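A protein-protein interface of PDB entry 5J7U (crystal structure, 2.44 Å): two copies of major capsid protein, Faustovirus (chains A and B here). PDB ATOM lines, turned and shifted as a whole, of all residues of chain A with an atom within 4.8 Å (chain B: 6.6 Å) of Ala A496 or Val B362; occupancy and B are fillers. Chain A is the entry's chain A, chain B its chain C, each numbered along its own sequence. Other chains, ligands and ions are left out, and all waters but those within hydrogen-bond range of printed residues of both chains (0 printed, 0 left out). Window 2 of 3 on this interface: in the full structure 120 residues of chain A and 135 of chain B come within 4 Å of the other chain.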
ATOM      1  N   ASP A 493     -23.257 -12.987  21.928  1.00  0.00           N
ATOM      2  CA  ASP A 493     -23.114 -11.674  21.305  1.00  0.00           C
ATOM      3  C   ASP A 493     -21.881 -11.554  20.417  1.00  0.00           C
ATOM      4  O   ASP A 493     -21.632 -10.463  19.891  1.00  0.00           O
ATOM      5  CB  ASP A 493     -23.080 -10.583  22.379  1.00  0.00           C
ATOM      6  CG  ASP A 493     -24.444 -10.323  22.993  1.00  0.00           C
ATOM      7  OD1 ASP A 493     -25.462 -10.694  22.369  1.00  0.00           O
ATOM      8  OD2 ASP A 493     -24.497  -9.738  24.094  1.00  0.00           O
ATOM      9  N   THR A 494     -21.107 -12.622  20.237  1.00  0.00           N
ATOM     10  CA  THR A 494     -19.949 -12.605  19.355  1.00  0.00           C
ATOM     11  C   THR A 494     -20.158 -13.432  18.093  1.00  0.00           C
ATOM     12  O   THR A 494     -19.257 -13.491  17.251  1.00  0.00           O
ATOM     13  CB  THR A 494     -18.702 -13.104  20.097  1.00  0.00           C
ATOM     14  OG1 THR A 494     -18.863 -14.487  20.438  1.00  0.00           O
ATOM     15  CG2 THR A 494     -18.485 -12.303  21.371  1.00  0.00           C
ATOM     16  N   VAL A 495     -21.318 -14.067  17.941  1.00  0.00           N
ATOM     17  CA  VAL A 495     -21.630 -14.900  16.787  1.00  0.00           C
ATOM     18  C   VAL A 495     -22.908 -14.377  16.149  1.00  0.00           C
ATOM     19  O   VAL A 495     -23.911 -14.171  16.842  1.00  0.00           O
ATOM     20  CB  VAL A 495     -21.785 -16.380  17.180  1.00  0.00           C
ATOM     21  CG1 VAL A 495     -22.138 -17.219  15.963  1.00  0.00           C
ATOM     22  CG2 VAL A 495     -20.516 -16.890  17.842  1.00  0.00           C
ATOM     23  N   ALA A 496     -22.872 -14.169  14.837  1.00  0.00           N
ATOM     24  CA  ALA A 496     -24.043 -13.677  14.125  1.00  0.00           C
ATOM     25  C   ALA A 496     -25.196 -14.670  14.263  1.00  0.00           C
ATOM     26  O   ALA A 496     -25.001 -15.873  14.037  1.00  0.00           O
ATOM     27  CB  ALA A 496     -23.714 -13.450  12.652  1.00  0.00           C
ATOM     28  N   PRO A 497     -26.399 -14.217  14.625  1.00  0.00           N
ATOM     29  CA  PRO A 497     -27.477 -15.182  14.901  1.00  0.00           C
ATOM     30  C   PRO A 497     -28.006 -15.888  13.666  1.00  0.00           C
ATOM     31  O   PRO A 497     -28.378 -17.065  13.751  1.00  0.00           O
ATOM     32  CB  PRO A 497     -28.551 -14.315  15.574  1.00  0.00           C
ATOM     33  CG  PRO A 497     -28.274 -12.922  15.081  1.00  0.00           C
ATOM     34  CD  PRO A 497     -26.785 -12.834  14.956  1.00  0.00           C
ATOM     35  N   VAL A 498     -28.047 -15.212  12.517  1.00  0.00           N
ATOM     36  CA  VAL A 498     -28.666 -15.795  11.331  1.00  0.00           C
ATOM     37  C   VAL A 498     -27.872 -17.016  10.892  1.00  0.00           C
ATOM     38  O   VAL A 498     -26.699 -16.912  10.512  1.00  0.00           O
ATOM     39  CB  VAL A 498     -28.769 -14.759  10.205  1.00  0.00           C
ATOM     40  CG1 VAL A 498     -29.412 -15.377   8.976  1.00  0.00           C
ATOM     41  CG2 VAL A 498     -29.560 -13.547  10.671  1.00  0.00           C
ATOM     42  N   SER A 500     -27.198 -19.636  12.907  1.00  0.00           N
ATOM     43  CA  SER A 500     -26.460 -20.189  14.032  1.00  0.00           C
ATOM     44  C   SER A 500     -27.398 -20.910  14.990  1.00  0.00           C
ATOM     45  O   SER A 500     -28.565 -20.539  15.143  1.00  0.00           O
ATOM     46  CB  SER A 500     -25.707 -19.086  14.783  1.00  0.00           C
ATOM     47  OG  SER A 500     -25.264 -19.540  16.050  1.00  0.00           O
ATOM     48  N   LEU B 350     -32.457  -6.649  15.344  1.00  0.00           N
ATOM     49  CA  LEU B 350     -31.795  -5.398  15.711  1.00  0.00           C
ATOM     50  C   LEU B 350     -30.423  -5.712  16.294  1.00  0.00           C
ATOM     51  O   LEU B 350     -30.323  -6.156  17.444  1.00  0.00           O
ATOM     52  CB  LEU B 350     -32.635  -4.601  16.705  1.00  0.00           C
ATOM     53  CG  LEU B 350     -31.968  -3.348  17.286  1.00  0.00           C
ATOM     54  CD1 LEU B 350     -31.713  -2.315  16.198  1.00  0.00           C
ATOM     55  CD2 LEU B 350     -32.803  -2.753  18.413  1.00  0.00           C
ATOM     56  N   THR B 351     -29.372  -5.468  15.517  1.00  0.00           N
ATOM     57  CA  THR B 351     -28.006  -5.672  15.974  1.00  0.00           C
ATOM     58  C   THR B 351     -27.282  -4.341  16.124  1.00  0.00           C
ATOM     59  O   THR B 351     -27.610  -3.351  15.462  1.00  0.00           O
ATOM     60  CB  THR B 351     -27.218  -6.576  15.020  1.00  0.00           C
ATOM     61  OG1 THR B 351     -27.479  -6.194  13.664  1.00  0.00           O
ATOM     62  CG2 THR B 351     -27.604  -8.031  15.222  1.00  0.00           C
ATOM     63  N   THR B 352     -26.283  -4.335  17.009  1.00  0.00           N
ATOM     64  CA  THR B 352     -25.493  -3.149  17.296  1.00  0.00           C
ATOM     65  C   THR B 352     -24.042  -3.262  16.860  1.00  0.00           C
ATOM     66  O   THR B 352     -23.389  -2.231  16.676  1.00  0.00           O
ATOM     67  CB  THR B 352     -25.526  -2.839  18.800  1.00  0.00           C
ATOM     68  OG1 THR B 352     -25.106  -3.998  19.534  1.00  0.00           O
ATOM     69  CG2 THR B 352     -26.929  -2.450  19.237  1.00  0.00           C
ATOM     70  N   GLY B 353     -23.526  -4.475  16.691  1.00  0.00           N
ATOM     71  CA  GLY B 353     -22.127  -4.680  16.383  1.00  0.00           C
ATOM     72  C   GLY B 353     -21.823  -4.560  14.904  1.00  0.00           C
ATOM     73  O   GLY B 353     -22.528  -3.893  14.141  1.00  0.00           O
ATOM     74  N   ALA B 354     -20.740  -5.216  14.499  1.00  0.00           N
ATOM     75  CA  ALA B 354     -20.332  -5.201  13.105  1.00  0.00           C
ATOM     76  C   ALA B 354     -21.352  -5.931  12.237  1.00  0.00           C
ATOM     77  O   ALA B 354     -21.982  -6.905  12.661  1.00  0.00           O
ATOM     78  CB  ALA B 354     -18.953  -5.839  12.942  1.00  0.00           C
ATOM     79  N   GLY B 355     -21.511  -5.444  11.008  1.00  0.00           N
ATOM     80  CA  GLY B 355     -22.480  -6.011  10.095  1.00  0.00           C
ATOM     81  C   GLY B 355     -23.924  -5.762  10.459  1.00  0.00           C
ATOM     82  O   GLY B 355     -24.808  -6.413   9.895  1.00  0.00           O
ATOM     83  N   LYS B 356     -24.189  -4.835  11.378  1.00  0.00           N
ATOM     84  CA  LYS B 356     -25.551  -4.589  11.834  1.00  0.00           C
ATOM     85  C   LYS B 356     -26.454  -4.229  10.659  1.00  0.00           C
ATOM     86  O   LYS B 356     -26.037  -3.588   9.690  1.00  0.00           O
ATOM     87  CB  LYS B 356     -25.574  -3.471  12.880  1.00  0.00           C
ATOM     88  CG  LYS B 356     -25.243  -2.087  12.345  1.00  0.00           C
ATOM     89  CD  LYS B 356     -25.458  -1.012  13.402  1.00  0.00           C
ATOM     90  CE  LYS B 356     -25.103   0.367  12.867  1.00  0.00           C
ATOM     91  NZ  LYS B 356     -25.227   1.421  13.911  1.00  0.00           N
ATOM     92  N   THR B 358     -27.594  -6.400   8.608  1.00  0.00           N
ATOM     93  CA  THR B 358     -27.386  -7.394   7.567  1.00  0.00           C
ATOM     94  C   THR B 358     -27.434  -8.784   8.188  1.00  0.00           C
ATOM     95  O   THR B 358     -27.492  -8.944   9.410  1.00  0.00           O
ATOM     96  CB  THR B 358     -26.048  -7.193   6.841  1.00  0.00           C
ATOM     97  OG1 THR B 358     -24.969  -7.510   7.730  1.00  0.00           O
ATOM     98  CG2 THR B 358     -25.903  -5.753   6.363  1.00  0.00           C
ATOM     99  N   ALA B 359     -27.397  -9.800   7.323  1.00  0.00           N
ATOM    100  CA  ALA B 359     -27.431 -11.181   7.789  1.00  0.00           C
ATOM    101  C   ALA B 359     -26.248 -11.525   8.687  1.00  0.00           C
ATOM    102  O   ALA B 359     -26.292 -12.544   9.384  1.00  0.00           O
ATOM    103  CB  ALA B 359     -27.468 -12.136   6.595  1.00  0.00           C
ATOM    104  N   THR B 360     -25.203 -10.697   8.695  1.00  0.00           N
ATOM    105  CA  THR B 360     -23.985 -10.971   9.447  1.00  0.00           C
ATOM    106  C   THR B 360     -23.854 -10.122  10.706  1.00  0.00           C
ATOM    107  O   THR B 360     -22.772 -10.091  11.306  1.00  0.00           O
ATOM    108  CB  THR B 360     -22.761 -10.758   8.554  1.00  0.00           C
ATOM    109  OG1 THR B 360     -22.803  -9.440   7.991  1.00  0.00           O
ATOM    110  CG2 THR B 360     -22.735 -11.786   7.430  1.00  0.00           C
ATOM    111  N   GLY B 361     -24.917  -9.439  11.127  1.00  0.00           N
ATOM    112  CA  GLY B 361     -24.823  -8.575  12.289  1.00  0.00           C
ATOM    113  C   GLY B 361     -24.575  -9.351  13.568  1.00  0.00           C
ATOM    114  O   GLY B 361     -24.986 -10.501  13.719  1.00  0.00           O
ATOM    115  N   VAL B 362     -23.894  -8.700  14.490  1.00  0.00           N
ATOM    116  CA  VAL B 362     -23.554  -9.279  15.766  1.00  0.00           C
ATOM    117  C   VAL B 362     -24.147  -8.506  16.908  1.00  0.00           C
ATOM    118  O   VAL B 362     -24.317  -7.336  16.821  1.00  0.00           O
ATOM    119  CB  VAL B 362     -22.039  -9.402  15.961  1.00  0.00           C
ATOM    120  CG1 VAL B 362     -21.512 -10.611  15.229  1.00  0.00           C
ATOM    121  CG2 VAL B 362     -21.327  -8.148  15.527  1.00  0.00           C
ATOM    122  N   LEU B 363     -24.460  -9.207  17.980  1.00  0.00           N
ATOM    123  CA  LEU B 363     -25.075  -8.638  19.165  1.00  0.00           C
ATOM    124  C   LEU B 363     -26.537  -8.315  18.884  1.00  0.00           C
ATOM    125  O   LEU B 363     -26.876  -7.247  18.443  1.00  0.00           O
ATOM    126  CB  LEU B 363     -24.304  -7.440  19.683  1.00  0.00           C
ATOM    127  CG  LEU B 363     -24.367  -7.350  21.193  1.00  0.00           C
ATOM    128  CD1 LEU B 363     -23.343  -6.392  21.731  1.00  0.00           C
ATOM    129  CD2 LEU B 363     -25.747  -6.917  21.621  1.00  0.00           C
ATOM    130  N   LEU B 364     -27.397  -9.275  19.160  1.00  0.00           N
ATOM    131  CA  LEU B 364     -28.817  -9.126  18.865  1.00  0.00           C
ATOM    132  C   LEU B 364     -29.550  -8.672  20.122  1.00  0.00           C
ATOM    133  O   LEU B 364     -29.547  -9.377  21.134  1.00  0.00           O
ATOM    134  CB  LEU B 364     -29.393 -10.447  18.355  1.00  0.00           C
ATOM    135  CG  LEU B 364     -30.913 -10.600  18.322  1.00  0.00           C
ATOM    136  CD1 LEU B 364     -31.532  -9.576  17.387  1.00  0.00           C
ATOM    137  CD2 LEU B 364     -31.279 -12.011  17.906  1.00  0.00           C
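N of Thr B352 sits at hydrogen-bond distance from O of Leu B363 (3.3 Å).
O of Val B362 sits at hydrogen-bond distance from N of Gly B353, at 3.0 Å.
The backbone NH of Val B362 lies close to the backbone carbonyl oxygen of Ala B354 (3.2 Å).
The backbone NH of Gly B361 sits close to the backbone carbonyl oxygen of Gly B355 (3.3 Å).
OG1 of Thr B358 sits at hydrogen-bond distance from OG1 of Thr B360 (2.9 Å).
Among the printed residues, merely in contact across the chains: Pro A497 with Gly B361 (3.2 Å), Ala A496 with Gly B361 (3.3 Å), Val A498 with Ala B359 (3.4 Å), Asp A493 with Leu B363 (3.5 Å), Ala A496 with Thr B360 (3.7 Å) and Ala A496 with Val B362 (3.8 Å).
Of chain B, only Thr B360, Gly B361 and Val B362 come within 4 Å of Ala A496.
Printed residues of chain B within 4 Å of Pro A497: Gly B361.
Printed residues of chain B within 4 Å of Val A498: Ala B359.
Of the printed residues of chain A, Gly B361 touches Ala A496 and Pro A497.
Of the printed residues of chain A, Ala B359 touches Val A498 (3.4 Å).
Printed residues of chain A within 4 Å of Thr B360: Ala A496 (3.7 Å).
The nearest residue of chain B that does not touch Ala A496 is Ala B359 (4.3 Å).
The nearest printed residue of chain A that does not touch Thr B360 is Val A498 (5.6 Å).
Of the 7 printed residues of chain A, 4 touch a printed residue of chain B.
Printed residues of chain A that touch a printed residue of chain B: Asp A493, Ala A496, Pro A497 and Val A498.
Hydrophobic or aromatic side chains of chain A within 4 Å of the printed part of chain B: Ala A496, Pro A497 and Val A498.
Among the printed residues, no Asp or Glu carboxylate lies within 4 Å of a Lys or Arg side-chain nitrogen of the other chain.
No position is printed for both chains.
Of the 6 pairs that touch across the chains among the printed residues, none has its exchanged pair printed and touching as well.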
